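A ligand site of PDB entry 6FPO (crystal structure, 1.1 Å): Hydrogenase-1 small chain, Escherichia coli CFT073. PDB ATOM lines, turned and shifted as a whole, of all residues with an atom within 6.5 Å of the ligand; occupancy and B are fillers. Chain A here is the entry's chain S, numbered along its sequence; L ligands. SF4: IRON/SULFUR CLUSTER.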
ATOM      1  N   ILE A 186       7.145 -23.399  26.689  1.00  0.00           N
ATOM      2  CA  ILE A 186       5.694 -23.512  26.660  1.00  0.00           C
ATOM      3  C   ILE A 186       5.187 -23.484  25.236  1.00  0.00           C
ATOM      4  O   ILE A 186       4.342 -24.300  24.811  1.00  0.00           O
ATOM      5  CB  ILE A 186       5.051 -22.355  27.518  1.00  0.00           C
ATOM      6  CG1 ILE A 186       5.379 -22.519  28.995  1.00  0.00           C
ATOM      7  CG2 ILE A 186       3.547 -22.218  27.253  1.00  0.00           C
ATOM      8  CD1 ILE A 186       4.784 -23.683  29.639  1.00  0.00           C
ATOM      9  N   HIS A 187       5.245 -22.531  24.404  1.00  0.00           N
ATOM     10  CA  HIS A 187       5.136 -22.144  22.994  1.00  0.00           C
ATOM     11  C   HIS A 187       5.590 -23.214  22.002  1.00  0.00           C
ATOM     12  O   HIS A 187       5.211 -23.171  20.828  1.00  0.00           O
ATOM     13  CB  HIS A 187       5.882 -20.842  22.740  1.00  0.00           C
ATOM     14  CG  HIS A 187       5.690 -20.292  21.363  1.00  0.00           C
ATOM     15  ND1 HIS A 187       4.479 -19.808  20.915  1.00  0.00           N
ATOM     16  CD2 HIS A 187       6.555 -20.142  20.332  1.00  0.00           C
ATOM     17  CE1 HIS A 187       4.605 -19.392  19.674  1.00  0.00           C
ATOM     18  NE2 HIS A 187       5.860 -19.582  19.292  1.00  0.00           N
ATOM     19  N   ASP A 188       6.608 -24.219  22.452  1.00  0.00           N
ATOM     20  CA  ASP A 188       6.951 -25.292  21.544  1.00  0.00           C
ATOM     21  C   ASP A 188       6.127 -26.565  21.791  1.00  0.00           C
ATOM     22  O   ASP A 188       6.323 -27.539  21.086  1.00  0.00           O
ATOM     23  CB  ASP A 188       8.466 -25.543  21.568  1.00  0.00           C
ATOM     24  CG  ASP A 188       9.274 -24.390  20.983  1.00  0.00           C
ATOM     25  OD1 ASP A 188       8.732 -23.610  20.159  1.00  0.00           O
ATOM     26  OD2 ASP A 188      10.438 -24.186  21.394  1.00  0.00           O
ATOM     27  N   CYS A 190       2.575 -25.853  22.718  1.00  0.00           N
ATOM     28  CA  CYS A 190       1.279 -25.210  22.961  1.00  0.00           C
ATOM     29  C   CYS A 190       0.261 -25.607  21.917  1.00  0.00           C
ATOM     30  O   CYS A 190       0.478 -25.463  20.709  1.00  0.00           O
ATOM     31  CB  CYS A 190       1.455 -23.678  22.976  1.00  0.00           C
ATOM     32  SG  CYS A 190      -0.135 -22.817  23.343  1.00  0.00           S
ATOM     33  N   TYR A 191      -0.898 -26.025  22.394  1.00  0.00           N
ATOM     34  CA  TYR A 191      -1.990 -26.442  21.487  1.00  0.00           C
ATOM     35  C   TYR A 191      -2.610 -25.310  20.692  1.00  0.00           C
ATOM     36  O   TYR A 191      -3.358 -25.607  19.773  1.00  0.00           O
ATOM     37  CB  TYR A 191      -3.067 -27.242  22.265  1.00  0.00           C
ATOM     38  CG  TYR A 191      -4.086 -26.419  22.995  1.00  0.00           C
ATOM     39  CD1 TYR A 191      -3.772 -25.397  23.904  1.00  0.00           C
ATOM     40  CD2 TYR A 191      -5.435 -26.642  22.769  1.00  0.00           C
ATOM     41  CE1 TYR A 191      -4.753 -24.647  24.532  1.00  0.00           C
ATOM     42  CE2 TYR A 191      -6.430 -25.901  23.383  1.00  0.00           C
ATOM     43  CZ  TYR A 191      -6.072 -24.866  24.249  1.00  0.00           C
ATOM     44  OH  TYR A 191      -7.019 -24.055  24.813  1.00  0.00           O
ATOM     45  N   ARG A 192      -2.264 -24.047  20.966  1.00  0.00           N
ATOM     46  CA  ARG A 192      -2.721 -22.941  20.142  1.00  0.00           C
ATOM     47  C   ARG A 192      -1.703 -22.519  19.087  1.00  0.00           C
ATOM     48  O   ARG A 192      -1.934 -21.531  18.365  1.00  0.00           O
ATOM     49  CB  ARG A 192      -3.181 -21.733  20.997  1.00  0.00           C
ATOM     50  CG  ARG A 192      -4.312 -22.097  21.925  1.00  0.00           C
ATOM     51  CD  ARG A 192      -4.893 -20.909  22.671  1.00  0.00           C
ATOM     52  NE  ARG A 192      -5.917 -21.314  23.605  1.00  0.00           N
ATOM     53  CZ  ARG A 192      -6.879 -20.527  24.071  1.00  0.00           C
ATOM     54  NH1 ARG A 192      -6.975 -19.273  23.705  1.00  0.00           N
ATOM     55  NH2 ARG A 192      -7.736 -21.056  24.941  1.00  0.00           N
ATOM     56  N   ARG A 193      -0.615 -23.284  18.949  1.00  0.00           N
ATOM     57  CA  ARG A 193       0.409 -22.879  18.016  1.00  0.00           C
ATOM     58  C   ARG A 193      -0.090 -22.853  16.557  1.00  0.00           C
ATOM     59  O   ARG A 193       0.390 -22.033  15.798  1.00  0.00           O
ATOM     60  CB  ARG A 193       1.603 -23.787  18.239  1.00  0.00           C
ATOM     61  CG  ARG A 193       2.820 -23.458  17.408  1.00  0.00           C
ATOM     62  CD  ARG A 193       3.452 -22.103  17.723  1.00  0.00           C
ATOM     63  NE  ARG A 193       4.610 -21.950  16.858  1.00  0.00           N
ATOM     64  CZ  ARG A 193       5.863 -22.294  17.173  1.00  0.00           C
ATOM     65  NH1 ARG A 193       6.227 -22.773  18.359  1.00  0.00           N
ATOM     66  NH2 ARG A 193       6.795 -22.128  16.254  1.00  0.00           N
ATOM     67  N   ALA A 194      -1.038 -23.707  16.190  1.00  0.00           N
ATOM     68  CA  ALA A 194      -1.608 -23.609  14.852  1.00  0.00           C
ATOM     69  C   ALA A 194      -2.102 -22.223  14.555  1.00  0.00           C
ATOM     70  O   ALA A 194      -1.997 -21.684  13.428  1.00  0.00           O
ATOM     71  CB  ALA A 194      -2.786 -24.577  14.696  1.00  0.00           C
ATOM     72  N   HIS A 195      -2.756 -21.616  15.549  1.00  0.00           N
ATOM     73  CA  HIS A 195      -3.303 -20.269  15.402  1.00  0.00           C
ATOM     74  C   HIS A 195      -2.185 -19.235  15.302  1.00  0.00           C
ATOM     75  O   HIS A 195      -2.243 -18.334  14.449  1.00  0.00           O
ATOM     76  CB  HIS A 195      -4.279 -19.945  16.517  1.00  0.00           C
ATOM     77  CG  HIS A 195      -5.420 -20.900  16.581  1.00  0.00           C
ATOM     78  ND1 HIS A 195      -6.250 -21.138  15.515  1.00  0.00           N
ATOM     79  CD2 HIS A 195      -5.861 -21.696  17.580  1.00  0.00           C
ATOM     80  CE1 HIS A 195      -7.170 -22.029  15.884  1.00  0.00           C
ATOM     81  NE2 HIS A 195      -6.969 -22.378  17.139  1.00  0.00           N
ATOM     82  N   PHE A 196      -1.166 -19.349  16.152  1.00  0.00           N
ATOM     83  CA  PHE A 196      -0.001 -18.460  16.018  1.00  0.00           C
ATOM     84  C   PHE A 196       0.547 -18.514  14.591  1.00  0.00           C
ATOM     85  O   PHE A 196       0.788 -17.490  13.956  1.00  0.00           O
ATOM     86  CB  PHE A 196       1.073 -18.894  17.019  1.00  0.00           C
ATOM     87  CG  PHE A 196       2.341 -18.088  16.982  1.00  0.00           C
ATOM     88  CD1 PHE A 196       2.477 -16.947  17.742  1.00  0.00           C
ATOM     89  CD2 PHE A 196       3.406 -18.460  16.203  1.00  0.00           C
ATOM     90  CE1 PHE A 196       3.625 -16.200  17.731  1.00  0.00           C
ATOM     91  CE2 PHE A 196       4.582 -17.741  16.245  1.00  0.00           C
ATOM     92  CZ  PHE A 196       4.690 -16.589  16.955  1.00  0.00           C
ATOM     93  N   PHE A 201      -5.278 -14.548  16.071  1.00  0.00           N
ATOM     94  CA  PHE A 201      -4.976 -14.023  17.396  1.00  0.00           C
ATOM     95  C   PHE A 201      -6.222 -13.439  18.047  1.00  0.00           C
ATOM     96  O   PHE A 201      -6.994 -12.722  17.422  1.00  0.00           O
ATOM     97  CB  PHE A 201      -3.943 -12.890  17.307  1.00  0.00           C
ATOM     98  CG  PHE A 201      -2.627 -13.314  16.754  1.00  0.00           C
ATOM     99  CD1 PHE A 201      -1.826 -14.177  17.411  1.00  0.00           C
ATOM    100  CD2 PHE A 201      -2.170 -12.846  15.510  1.00  0.00           C
ATOM    101  CE1 PHE A 201      -0.627 -14.601  16.928  1.00  0.00           C
ATOM    102  CE2 PHE A 201      -0.967 -13.229  15.024  1.00  0.00           C
ATOM    103  CZ  PHE A 201      -0.153 -14.096  15.713  1.00  0.00           C
ATOM    104  N   TYR A 214      -8.169 -18.929  19.927  1.00  0.00           N
ATOM    105  CA  TYR A 214      -7.042 -18.451  19.168  1.00  0.00           C
ATOM    106  C   TYR A 214      -5.859 -18.084  20.067  1.00  0.00           C
ATOM    107  O   TYR A 214      -5.943 -18.022  21.295  1.00  0.00           O
ATOM    108  CB  TYR A 214      -7.469 -17.278  18.257  1.00  0.00           C
ATOM    109  CG  TYR A 214      -8.239 -17.678  17.017  1.00  0.00           C
ATOM    110  CD1 TYR A 214      -8.676 -18.961  16.754  1.00  0.00           C
ATOM    111  CD2 TYR A 214      -8.539 -16.702  16.058  1.00  0.00           C
ATOM    112  CE1 TYR A 214      -9.373 -19.294  15.593  1.00  0.00           C
ATOM    113  CE2 TYR A 214      -9.199 -17.050  14.911  1.00  0.00           C
ATOM    114  CZ  TYR A 214      -9.677 -18.324  14.730  1.00  0.00           C
ATOM    115  OH  TYR A 214     -10.359 -18.578  13.528  1.00  0.00           O
ATOM    116  N   CYS A 215      -4.706 -17.887  19.425  1.00  0.00           N
ATOM    117  CA  CYS A 215      -3.470 -17.613  20.118  1.00  0.00           C
ATOM    118  C   CYS A 215      -3.534 -16.307  20.891  1.00  0.00           C
ATOM    119  O   CYS A 215      -4.162 -15.329  20.434  1.00  0.00           O
ATOM    120  CB  CYS A 215      -2.333 -17.670  19.120  1.00  0.00           C
ATOM    121  SG  CYS A 215      -0.725 -17.047  19.718  1.00  0.00           S
ATOM    122  N   LEU A 216      -2.856 -16.280  22.039  1.00  0.00           N
ATOM    123  CA  LEU A 216      -2.814 -15.168  22.995  1.00  0.00           C
ATOM    124  C   LEU A 216      -1.585 -14.289  22.871  1.00  0.00           C
ATOM    125  O   LEU A 216      -1.369 -13.418  23.720  1.00  0.00           O
ATOM    126  CB  LEU A 216      -2.989 -15.737  24.409  1.00  0.00           C
ATOM    127  CG  LEU A 216      -4.305 -16.464  24.597  1.00  0.00           C
ATOM    128  CD1 LEU A 216      -4.331 -17.225  25.889  1.00  0.00           C
ATOM    129  CD2 LEU A 216      -5.488 -15.603  24.497  1.00  0.00           C
ATOM    130  N   TYR A 217      -0.789 -14.454  21.816  1.00  0.00           N
ATOM    131  CA  TYR A 217       0.430 -13.648  21.636  1.00  0.00           C
ATOM    132  C   TYR A 217       0.177 -12.151  21.692  1.00  0.00           C
ATOM    133  O   TYR A 217       0.924 -11.407  22.353  1.00  0.00           O
ATOM    134  CB  TYR A 217       1.067 -14.014  20.295  1.00  0.00           C
ATOM    135  CG  TYR A 217       2.207 -13.207  19.902  1.00  0.00           C
ATOM    136  CD1 TYR A 217       3.412 -13.355  20.528  1.00  0.00           C
ATOM    137  CD2 TYR A 217       2.077 -12.273  18.895  1.00  0.00           C
ATOM    138  CE1 TYR A 217       4.511 -12.621  20.150  1.00  0.00           C
ATOM    139  CE2 TYR A 217       3.120 -11.471  18.530  1.00  0.00           C
ATOM    140  CZ  TYR A 217       4.328 -11.695  19.184  1.00  0.00           C
ATOM    141  OH  TYR A 217       5.493 -10.974  18.851  1.00  0.00           O
ATOM    142  N   LYS A 218      -0.860 -11.669  21.005  1.00  0.00           N
ATOM    143  CA  LYS A 218      -1.142 -10.242  20.996  1.00  0.00           C
ATOM    144  C   LYS A 218      -1.728  -9.743  22.294  1.00  0.00           C
ATOM    145  O   LYS A 218      -1.754  -8.519  22.528  1.00  0.00           O
ATOM    146  CB  LYS A 218      -2.001  -9.838  19.803  1.00  0.00           C
ATOM    147  CG  LYS A 218      -1.357 -10.092  18.486  1.00  0.00           C
ATOM    148  CD  LYS A 218      -2.105  -9.452  17.341  1.00  0.00           C
ATOM    149  CE  LYS A 218      -1.305  -9.508  16.077  1.00  0.00           C
ATOM    150  NZ  LYS A 218      -2.086  -8.998  14.909  1.00  0.00           N
ATOM    151  N   CYS A 221       1.028 -13.012  25.779  1.00  0.00           N
ATOM    152  CA  CYS A 221       1.526 -14.324  26.205  1.00  0.00           C
ATOM    153  C   CYS A 221       3.047 -14.387  26.123  1.00  0.00           C
ATOM    154  O   CYS A 221       3.639 -14.125  25.060  1.00  0.00           O
ATOM    155  CB  CYS A 221       0.958 -15.390  25.260  1.00  0.00           C
ATOM    156  SG  CYS A 221       1.388 -17.062  25.769  1.00  0.00           S
ATOM    157  N   LYS A 222       3.666 -14.840  27.210  1.00  0.00           N
ATOM    158  CA  LYS A 222       5.126 -14.991  27.276  1.00  0.00           C
ATOM    159  C   LYS A 222       5.559 -16.422  27.081  1.00  0.00           C
ATOM    160  O   LYS A 222       6.730 -16.777  27.303  1.00  0.00           O
ATOM    161  CB  LYS A 222       5.674 -14.418  28.583  1.00  0.00           C
ATOM    162  CG  LYS A 222       5.337 -12.912  28.746  1.00  0.00           C
ATOM    163  CD  LYS A 222       5.695 -12.069  27.479  1.00  0.00           C
ATOM    164  CE  LYS A 222       5.585 -10.594  27.547  1.00  0.00           C
ATOM    165  NZ  LYS A 222       4.316 -10.098  28.152  1.00  0.00           N
ATOM    166  N   GLY A 223       4.671 -17.289  26.591  1.00  0.00           N
ATOM    167  CA  GLY A 223       5.032 -18.639  26.267  1.00  0.00           C
ATOM    168  C   GLY A 223       6.259 -18.795  25.376  1.00  0.00           C
ATOM    169  O   GLY A 223       7.061 -19.724  25.581  1.00  0.00           O
ATOM    170  N   PRO A 224       6.462 -17.866  24.402  1.00  0.00           N
ATOM    171  CA  PRO A 224       7.651 -18.018  23.528  1.00  0.00           C
ATOM    172  C   PRO A 224       8.994 -17.920  24.210  1.00  0.00           C
ATOM    173  O   PRO A 224       9.999 -18.299  23.594  1.00  0.00           O
ATOM    174  CB  PRO A 224       7.470 -16.877  22.495  1.00  0.00           C
ATOM    175  CG  PRO A 224       5.992 -16.762  22.399  1.00  0.00           C
ATOM    176  CD  PRO A 224       5.504 -16.908  23.838  1.00  0.00           C
ATOM    177  N   PHE A 241      -4.372 -25.217  31.904  1.00  0.00           N
ATOM    178  CA  PHE A 241      -3.181 -24.424  32.171  1.00  0.00           C
ATOM    179  C   PHE A 241      -3.554 -22.997  31.802  1.00  0.00           C
ATOM    180  O   PHE A 241      -4.617 -22.750  31.222  1.00  0.00           O
ATOM    181  CB  PHE A 241      -1.914 -24.946  31.463  1.00  0.00           C
ATOM    182  CG  PHE A 241      -1.781 -24.718  29.991  1.00  0.00           C
ATOM    183  CD1 PHE A 241      -2.565 -25.391  29.089  1.00  0.00           C
ATOM    184  CD2 PHE A 241      -0.755 -23.917  29.501  1.00  0.00           C
ATOM    185  CE1 PHE A 241      -2.336 -25.241  27.712  1.00  0.00           C
ATOM    186  CE2 PHE A 241      -0.532 -23.784  28.150  1.00  0.00           C
ATOM    187  CZ  PHE A 241      -1.345 -24.478  27.258  1.00  0.00           C
ATOM    188  N   ILE A 243      -3.022 -20.719  29.469  1.00  0.00           N
ATOM    189  CA  ILE A 243      -3.428 -20.427  28.099  1.00  0.00           C
ATOM    190  C   ILE A 243      -4.726 -21.146  27.767  1.00  0.00           C
ATOM    191  O   ILE A 243      -5.589 -20.603  27.088  1.00  0.00           O
ATOM    192  CB  ILE A 243      -2.283 -20.816  27.155  1.00  0.00           C
ATOM    193  CG1 ILE A 243      -1.146 -19.802  27.259  1.00  0.00           C
ATOM    194  CG2 ILE A 243      -2.734 -20.975  25.696  1.00  0.00           C
ATOM    195  CD1 ILE A 243       0.226 -20.367  27.025  1.00  0.00           C
ATOM    196  N   GLY A 248      -2.784 -15.340  28.589  1.00  0.00           N
ATOM    197  CA  GLY A 248      -1.436 -15.651  28.201  1.00  0.00           C
ATOM    198  C   GLY A 248      -0.566 -16.067  29.368  1.00  0.00           C
ATOM    199  O   GLY A 248      -0.781 -15.658  30.527  1.00  0.00           O
ATOM    200  N   CYS A 249       0.470 -16.840  29.081  1.00  0.00           N
ATOM    201  CA  CYS A 249       1.527 -17.095  30.036  1.00  0.00           C
ATOM    202  C   CYS A 249       2.100 -15.763  30.519  1.00  0.00           C
ATOM    203  O   CYS A 249       2.352 -14.854  29.730  1.00  0.00           O
ATOM    204  CB  CYS A 249       2.580 -17.993  29.364  1.00  0.00           C
ATOM    205  SG  CYS A 249       4.077 -18.360  30.286  1.00  0.00           S
HETATM  206 FE1  SF4 L   1       0.205 -18.452  21.261  1.00  0.00          FE
HETATM  207 FE2  SF4 L   1       1.209 -18.273  23.815  1.00  0.00          FE
HETATM  208 FE3  SF4 L   1       2.669 -19.431  21.820  1.00  0.00          FE
HETATM  209 FE4  SF4 L   1       0.488 -20.696  22.792  1.00  0.00          FE
HETATM  210  S1  SF4 L   1       2.445 -20.199  23.944  1.00  0.00           S
HETATM  211  S2  SF4 L   1       1.012 -20.471  20.576  1.00  0.00           S
HETATM  212  S3  SF4 L   1      -0.935 -18.939  23.178  1.00  0.00           S
HETATM  213  S4  SF4 L   1       2.051 -17.234  21.960  1.00  0.00           S
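FE1 of the ligand is bound by SG of Cys 215, at 2.3 Å.
A sulfur (S1) of the ligand sits close to the backbone NH (N) of His 187, 3.7 Å away.
The backbone NH of Arg 193 sits close to a sulfur (S2) of the ligand (3.6 Å).
An iron atom (FE2) of the ligand is bound by the side-chain sulfur (SG) of Cys 221.
SG of Cys 190 is bound to FE4 of the ligand, 2.3 Å away.
A ring nitrogen (ND1) of His 187 binds an iron atom (FE3) of the ligand (2.1 Å).
S3 of the ligand lies close to N of Leu 216, 3.5 Å away.
Arg 192 touches the ligand (C to S2, 3.7 Å).
Phe 196 touches the ligand.
Tyr 217 touches the ligand.
Gly 223 touches the ligand.
CD of Pro 224 touches S4 of the ligand, at 3.9 Å.
CG2 of Ile 243 touches S3 of the ligand, 3.7 Å away.
Hydrophobic or aromatic side chains that line the ligand: His 187, Phe 196, Leu 216, Tyr 217, Pro 224 and Ile 243.
Of the 24 residues printed, 12 come within 4 Å of the ligand.
The nearest printed residue that does not touch the ligand is Ile 186 (4.03 Å).
SG of Cys 190 sits close to N of Arg 192 (3.4 Å).
The guanidinium group (NH2) of Arg 192 is in hydrogen-bond range of the side-chain hydroxyl (OH) of Tyr 191, 3.1 Å away.
The backbone carbonyl oxygen (O) of Ile 243 sits at hydrogen-bond distance from the guanidinium group (NH2) of Arg 192 (3.1 Å).
N of Cys 221 lies within hydrogen-bond range of O of Leu 216 (3.2 Å).
The backbone carbonyl oxygen of Tyr 214 is in hydrogen-bond range of the guanidinium group of Arg 192, at 2.9 Å.
The guanidinium group (NH1) of Arg 193 sits at hydrogen-bond distance from the backbone carbonyl oxygen (O) of His 187 (2.7 Å).
SG of Cys 221 sits close to N of Cys 249.
N of Gly 223 lies close to SG of Cys 221 (3.4 Å).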
